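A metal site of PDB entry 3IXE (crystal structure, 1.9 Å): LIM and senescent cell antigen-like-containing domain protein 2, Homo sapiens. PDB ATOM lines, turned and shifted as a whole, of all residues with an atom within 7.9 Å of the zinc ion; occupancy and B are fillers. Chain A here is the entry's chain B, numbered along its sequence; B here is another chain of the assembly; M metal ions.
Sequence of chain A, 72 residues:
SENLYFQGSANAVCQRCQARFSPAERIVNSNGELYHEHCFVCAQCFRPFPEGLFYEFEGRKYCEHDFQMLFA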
ATOM      1  N   VAL A  41      14.338   8.421 -29.031  1.00  0.00           N
ATOM      2  CA  VAL A  41      13.424   7.329 -29.371  1.00  0.00           C
ATOM      3  C   VAL A  41      13.693   6.161 -28.426  1.00  0.00           C
ATOM      4  O   VAL A  41      14.706   6.143 -27.734  1.00  0.00           O
ATOM      5  CB  VAL A  41      13.638   6.822 -30.832  1.00  0.00           C
ATOM      6  CG1 VAL A  41      13.275   7.879 -31.871  1.00  0.00           C
ATOM      7  CG2 VAL A  41      15.086   6.292 -31.040  1.00  0.00           C
ATOM      8  N   CYS A  42      12.788   5.195 -28.410  1.00  0.00           N
ATOM      9  CA  CYS A  42      12.969   4.004 -27.578  1.00  0.00           C
ATOM     10  C   CYS A  42      14.162   3.185 -28.062  1.00  0.00           C
ATOM     11  O   CYS A  42      14.346   2.985 -29.265  1.00  0.00           O
ATOM     12  CB  CYS A  42      11.702   3.163 -27.589  1.00  0.00           C
ATOM     13  SG  CYS A  42      11.827   1.596 -26.736  1.00  0.00           S
ATOM     14  N   ALA A  43      14.998   2.743 -27.119  1.00  0.00           N
ATOM     15  CA  ALA A  43      16.198   1.958 -27.436  1.00  0.00           C
ATOM     16  C   ALA A  43      15.832   0.608 -28.023  1.00  0.00           C
ATOM     17  O   ALA A  43      16.591   0.052 -28.812  1.00  0.00           O
ATOM     18  CB  ALA A  43      17.045   1.771 -26.186  1.00  0.00           C
ATOM     19  N   GLN A  44      14.653   0.095 -27.664  1.00  0.00           N
ATOM     20  CA  GLN A  44      14.206  -1.216 -28.116  1.00  0.00           C
ATOM     21  C   GLN A  44      13.523  -1.220 -29.484  1.00  0.00           C
ATOM     22  O   GLN A  44      13.863  -2.043 -30.330  1.00  0.00           O
ATOM     23  CB  GLN A  44      13.311  -1.883 -27.063  1.00  0.00           C
ATOM     24  CG  GLN A  44      13.144  -3.403 -27.246  1.00  0.00           C
ATOM     25  CD  GLN A  44      14.438  -4.175 -27.030  1.00  0.00           C
ATOM     26  OE1 GLN A  44      15.409  -3.643 -26.484  1.00  0.00           O
ATOM     27  NE2 GLN A  44      14.450  -5.439 -27.439  1.00  0.00           N
ATOM     28  N   CYS A  45      12.574  -0.318 -29.712  1.00  0.00           N
ATOM     29  CA  CYS A  45      11.797  -0.319 -30.962  1.00  0.00           C
ATOM     30  C   CYS A  45      12.179   0.795 -31.933  1.00  0.00           C
ATOM     31  O   CYS A  45      11.729   0.792 -33.075  1.00  0.00           O
ATOM     32  CB  CYS A  45      10.296  -0.246 -30.664  1.00  0.00           C
ATOM     33  SG  CYS A  45       9.792   1.301 -29.857  1.00  0.00           S
ATOM     34  N   PHE A  46      12.993   1.743 -31.455  1.00  0.00           N
ATOM     35  CA  PHE A  46      13.464   2.925 -32.218  1.00  0.00           C
ATOM     36  C   PHE A  46      12.388   3.933 -32.596  1.00  0.00           C
ATOM     37  O   PHE A  46      12.629   4.828 -33.429  1.00  0.00           O
ATOM     38  CB  PHE A  46      14.271   2.568 -33.487  1.00  0.00           C
ATOM     39  CG  PHE A  46      15.211   1.398 -33.344  1.00  0.00           C
ATOM     40  CD1 PHE A  46      16.108   1.319 -32.275  1.00  0.00           C
ATOM     41  CD2 PHE A  46      15.222   0.390 -34.299  1.00  0.00           C
ATOM     42  CE1 PHE A  46      16.984   0.233 -32.160  1.00  0.00           C
ATOM     43  CE2 PHE A  46      16.114  -0.687 -34.196  1.00  0.00           C
ATOM     44  CZ  PHE A  46      16.987  -0.770 -33.120  1.00  0.00           C
ATOM     45  N   ARG A  47      11.199   3.824 -31.988  1.00  0.00           N
ATOM     46  CA  ARG A  47      10.113   4.738 -32.330  1.00  0.00           C
ATOM     47  C   ARG A  47      10.080   5.953 -31.397  1.00  0.00           C
ATOM     48  O   ARG A  47      10.491   5.851 -30.247  1.00  0.00           O
ATOM     49  CB  ARG A  47       8.751   4.029 -32.324  1.00  0.00           C
ATOM     50  CG  ARG A  47       8.671   2.697 -33.079  1.00  0.00           C
ATOM     51  CD  ARG A  47       9.219   2.772 -34.497  1.00  0.00           C
ATOM     52  NE  ARG A  47       8.520   3.762 -35.314  1.00  0.00           N
ATOM     53  CZ  ARG A  47       8.849   4.056 -36.576  1.00  0.00           C
ATOM     54  NH1 ARG A  47       9.863   3.440 -37.167  1.00  0.00           N
ATOM     55  NH2 ARG A  47       8.147   4.968 -37.241  1.00  0.00           N
ATOM     56  N   PRO A  48       9.570   7.094 -31.891  1.00  0.00           N
ATOM     57  CA  PRO A  48       9.330   8.216 -30.988  1.00  0.00           C
ATOM     58  C   PRO A  48       8.394   7.775 -29.863  1.00  0.00           C
ATOM     59  O   PRO A  48       7.536   6.917 -30.079  1.00  0.00           O
ATOM     60  CB  PRO A  48       8.642   9.255 -31.884  1.00  0.00           C
ATOM     61  CG  PRO A  48       9.082   8.930 -33.256  1.00  0.00           C
ATOM     62  CD  PRO A  48       9.222   7.428 -33.289  1.00  0.00           C
ATOM     63  N   PHE A  49       8.589   8.343 -28.683  1.00  0.00           N
ATOM     64  CA  PHE A  49       7.828   7.932 -27.508  1.00  0.00           C
ATOM     65  C   PHE A  49       6.386   8.402 -27.633  1.00  0.00           C
ATOM     66  O   PHE A  49       6.137   9.605 -27.772  1.00  0.00           O
ATOM     67  CB  PHE A  49       8.451   8.523 -26.230  1.00  0.00           C
ATOM     68  CG  PHE A  49       9.890   8.133 -26.011  1.00  0.00           C
ATOM     69  CD1 PHE A  49      10.229   6.807 -25.747  1.00  0.00           C
ATOM     70  CD2 PHE A  49      10.899   9.084 -26.058  1.00  0.00           C
ATOM     71  CE1 PHE A  49      11.565   6.443 -25.542  1.00  0.00           C
ATOM     72  CE2 PHE A  49      12.234   8.732 -25.860  1.00  0.00           C
ATOM     73  CZ  PHE A  49      12.571   7.412 -25.589  1.00  0.00           C
ATOM     74  N   PRO A  50       5.420   7.457 -27.614  1.00  0.00           N
ATOM     75  CA  PRO A  50       4.011   7.901 -27.585  1.00  0.00           C
ATOM     76  C   PRO A  50       3.738   8.805 -26.384  1.00  0.00           C
ATOM     77  O   PRO A  50       4.101   8.441 -25.248  1.00  0.00           O
ATOM     78  CB  PRO A  50       3.217   6.594 -27.466  1.00  0.00           C
ATOM     79  CG  PRO A  50       4.141   5.539 -27.980  1.00  0.00           C
ATOM     80  CD  PRO A  50       5.529   5.991 -27.631  1.00  0.00           C
ATOM     81  N   LYS A  61      16.687   4.637 -22.737  1.00  0.00           N
ATOM     82  CA  LYS A  61      15.315   5.080 -22.645  1.00  0.00           C
ATOM     83  C   LYS A  61      14.390   4.126 -23.392  1.00  0.00           C
ATOM     84  O   LYS A  61      14.704   3.704 -24.516  1.00  0.00           O
ATOM     85  CB  LYS A  61      15.163   6.488 -23.227  1.00  0.00           C
ATOM     86  CG  LYS A  61      15.941   7.573 -22.491  1.00  0.00           C
ATOM     87  CD  LYS A  61      15.752   8.919 -23.192  1.00  0.00           C
ATOM     88  CE  LYS A  61      16.295  10.070 -22.365  1.00  0.00           C
ATOM     89  NZ  LYS A  61      17.770  10.000 -22.211  1.00  0.00           N
ATOM     90  N   TYR A  62      13.245   3.807 -22.791  1.00  0.00           N
ATOM     91  CA  TYR A  62      12.306   2.831 -23.341  1.00  0.00           C
ATOM     92  C   TYR A  62      10.889   3.338 -23.282  1.00  0.00           C
ATOM     93  O   TYR A  62      10.517   4.057 -22.364  1.00  0.00           O
ATOM     94  CB  TYR A  62      12.396   1.506 -22.573  1.00  0.00           C
ATOM     95  CG  TYR A  62      13.755   0.857 -22.618  1.00  0.00           C
ATOM     96  CD1 TYR A  62      14.107  -0.021 -23.636  1.00  0.00           C
ATOM     97  CD2 TYR A  62      14.710   1.130 -21.630  1.00  0.00           C
ATOM     98  CE1 TYR A  62      15.356  -0.616 -23.679  1.00  0.00           C
ATOM     99  CE2 TYR A  62      15.970   0.555 -21.669  1.00  0.00           C
ATOM    100  CZ  TYR A  62      16.285  -0.317 -22.691  1.00  0.00           C
ATOM    101  OH  TYR A  62      17.520  -0.913 -22.736  1.00  0.00           O
ATOM    102  N   CYS A  63      10.092   2.958 -24.286  1.00  0.00           N
ATOM    103  CA  CYS A  63       8.664   3.254 -24.276  1.00  0.00           C
ATOM    104  C   CYS A  63       7.991   2.373 -23.231  1.00  0.00           C
ATOM    105  O   CYS A  63       8.574   1.394 -22.772  1.00  0.00           O
ATOM    106  CB  CYS A  63       8.066   3.006 -25.676  1.00  0.00           C
ATOM    107  SG  CYS A  63       7.992   1.259 -26.213  1.00  0.00           S
ATOM    108  N   GLU A  64       6.752   2.703 -22.859  1.00  0.00           N
ATOM    109  CA  GLU A  64       6.028   1.891 -21.890  1.00  0.00           C
ATOM    110  C   GLU A  64       5.956   0.411 -22.280  1.00  0.00           C
ATOM    111  O   GLU A  64       6.234  -0.469 -21.450  1.00  0.00           O
ATOM    112  CB  GLU A  64       4.636   2.446 -21.618  1.00  0.00           C
ATOM    113  CG  GLU A  64       4.014   1.826 -20.383  1.00  0.00           C
ATOM    114  CD  GLU A  64       3.031   2.736 -19.691  1.00  0.00           C
ATOM    115  OE1 GLU A  64       1.915   2.889 -20.208  1.00  0.00           O
ATOM    116  OE2 GLU A  64       3.387   3.293 -18.626  1.00  0.00           O
ATOM    117  N   HIS A  65       5.599   0.130 -23.531  1.00  0.00           N
ATOM    118  CA  HIS A  65       5.465  -1.241 -24.002  1.00  0.00           C
ATOM    119  C   HIS A  65       6.736  -2.058 -23.726  1.00  0.00           C
ATOM    120  O   HIS A  65       6.690  -3.098 -23.082  1.00  0.00           O
ATOM    121  CB  HIS A  65       5.147  -1.280 -25.501  1.00  0.00           C
ATOM    122  CG  HIS A  65       5.131  -2.670 -26.060  1.00  0.00           C
ATOM    123  ND1 HIS A  65       4.080  -3.535 -25.884  1.00  0.00           N
ATOM    124  CD2 HIS A  65       6.061  -3.359 -26.778  1.00  0.00           C
ATOM    125  CE1 HIS A  65       4.347  -4.681 -26.477  1.00  0.00           C
ATOM    126  NE2 HIS A  65       5.548  -4.606 -27.021  1.00  0.00           N
ATOM    127  N   ASP A  66       7.856  -1.575 -24.259  1.00  0.00           N
ATOM    128  CA  ASP A  66       9.128  -2.273 -24.149  1.00  0.00           C
ATOM    129  C   ASP A  66       9.662  -2.360 -22.719  1.00  0.00           C
ATOM    130  O   ASP A  66      10.189  -3.405 -22.322  1.00  0.00           O
ATOM    131  CB  ASP A  66      10.144  -1.648 -25.097  1.00  0.00           C
ATOM    132  CG  ASP A  66       9.876  -2.054 -26.534  1.00  0.00           C
ATOM    133  OD1 ASP A  66       9.599  -3.250 -26.746  1.00  0.00           O
ATOM    134  OD2 ASP A  66       9.927  -1.197 -27.441  1.00  0.00           O
ATOM    135  N   PHE A  67       9.512  -1.288 -21.953  1.00  0.00           N
ATOM    136  CA  PHE A  67       9.893  -1.333 -20.552  1.00  0.00           C
ATOM    137  C   PHE A  67       9.118  -2.406 -19.773  1.00  0.00           C
ATOM    138  O   PHE A  67       9.708  -3.189 -19.019  1.00  0.00           O
ATOM    139  CB  PHE A  67       9.756   0.040 -19.895  1.00  0.00           C
ATOM    140  CG  PHE A  67      10.242   0.057 -18.475  1.00  0.00           C
ATOM    141  CD1 PHE A  67      11.609   0.128 -18.190  1.00  0.00           C
ATOM    142  CD2 PHE A  67       9.335  -0.041 -17.421  1.00  0.00           C
ATOM    143  CE1 PHE A  67      12.068   0.124 -16.865  1.00  0.00           C
ATOM    144  CE2 PHE A  67       9.792  -0.039 -16.089  1.00  0.00           C
ATOM    145  CZ  PHE A  67      11.152   0.048 -15.816  1.00  0.00           C
ATOM    146  N   LEU A  70      10.210  -6.001 -20.924  1.00  0.00           N
ATOM    147  CA  LEU A  70      11.581  -6.413 -20.625  1.00  0.00           C
ATOM    148  C   LEU A  70      12.098  -6.194 -19.207  1.00  0.00           C
ATOM    149  O   LEU A  70      12.802  -7.052 -18.677  1.00  0.00           O
ATOM    150  CB  LEU A  70      12.559  -5.752 -21.622  1.00  0.00           C
ATOM    151  CG  LEU A  70      12.336  -6.029 -23.106  1.00  0.00           C
ATOM    152  CD1 LEU A  70      13.314  -5.189 -23.923  1.00  0.00           C
ATOM    153  CD2 LEU A  70      12.475  -7.498 -23.435  1.00  0.00           C
ATOM    154  N   HIS B 104       9.770  -6.773 -32.735  1.00  0.00           N
ATOM    155  CA  HIS B 104       9.691  -5.579 -33.598  1.00  0.00           C
ATOM    156  C   HIS B 104      10.237  -5.843 -34.990  1.00  0.00           C
ATOM    157  O   HIS B 104      10.291  -4.934 -35.818  1.00  0.00           O
ATOM    158  CB  HIS B 104      10.442  -4.421 -32.945  1.00  0.00           C
ATOM    159  CG  HIS B 104       9.927  -4.065 -31.580  1.00  0.00           C
ATOM    160  ND1 HIS B 104       8.668  -3.555 -31.385  1.00  0.00           N
ATOM    161  CD2 HIS B 104      10.499  -4.174 -30.361  1.00  0.00           C
ATOM    162  CE1 HIS B 104       8.469  -3.353 -30.088  1.00  0.00           C
ATOM    163  NE2 HIS B 104       9.563  -3.732 -29.440  1.00  0.00           N
ATOM    164  N   TYR B 137       8.554  -2.051 -38.877  1.00  0.00           N
ATOM    165  CA  TYR B 137       8.200  -0.641 -39.065  1.00  0.00           C
ATOM    166  C   TYR B 137       8.980  -0.012 -40.230  1.00  0.00           C
ATOM    167  O   TYR B 137       9.133   1.211 -40.314  1.00  0.00           O
ATOM    168  CB  TYR B 137       8.410   0.143 -37.763  1.00  0.00           C
ATOM    169  CG  TYR B 137       8.001  -0.657 -36.550  1.00  0.00           C
ATOM    170  CD1 TYR B 137       6.703  -1.160 -36.436  1.00  0.00           C
ATOM    171  CD2 TYR B 137       8.921  -0.937 -35.526  1.00  0.00           C
ATOM    172  CE1 TYR B 137       6.319  -1.938 -35.342  1.00  0.00           C
ATOM    173  CE2 TYR B 137       8.541  -1.714 -34.419  1.00  0.00           C
ATOM    174  CZ  TYR B 137       7.237  -2.211 -34.348  1.00  0.00           C
ATOM    175  OH  TYR B 137       6.819  -2.976 -33.274  1.00  0.00           O
HETATM  176 ZN    ZN M   1       9.818   0.789 -27.573  1.00  0.00          ZN
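A ring nitrogen (NE2) of His 104 of chain B lies within hydrogen-bond range of the side-chain carboxylate (OD1) of Asp 66, 2.7 Å away.
The side-chain sulfur (SG) of Cys 42 sits close to the backbone NH (N) of Gln 44 (3.3 Å).
O of Arg 47 is in hydrogen-bond range of N of Cys 42 (3.0 Å).
SG of Cys 63 sits close to N of His 65, 3.8 Å away.
The side-chain sulfur (SG) of Cys 45 lies close to the backbone NH (N) of Arg 47 (3.6 Å).
The zinc ion is bound by the side-chain carboxylate of Asp 66 (2.0 Å), the side-chain sulfur of Cys 42 (2.3 Å), the side-chain sulfur of Cys 63 (2.3 Å) and the side-chain sulfur of Cys 45 (2.3 Å).
The zinc ion has four donor atoms within binding distance.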
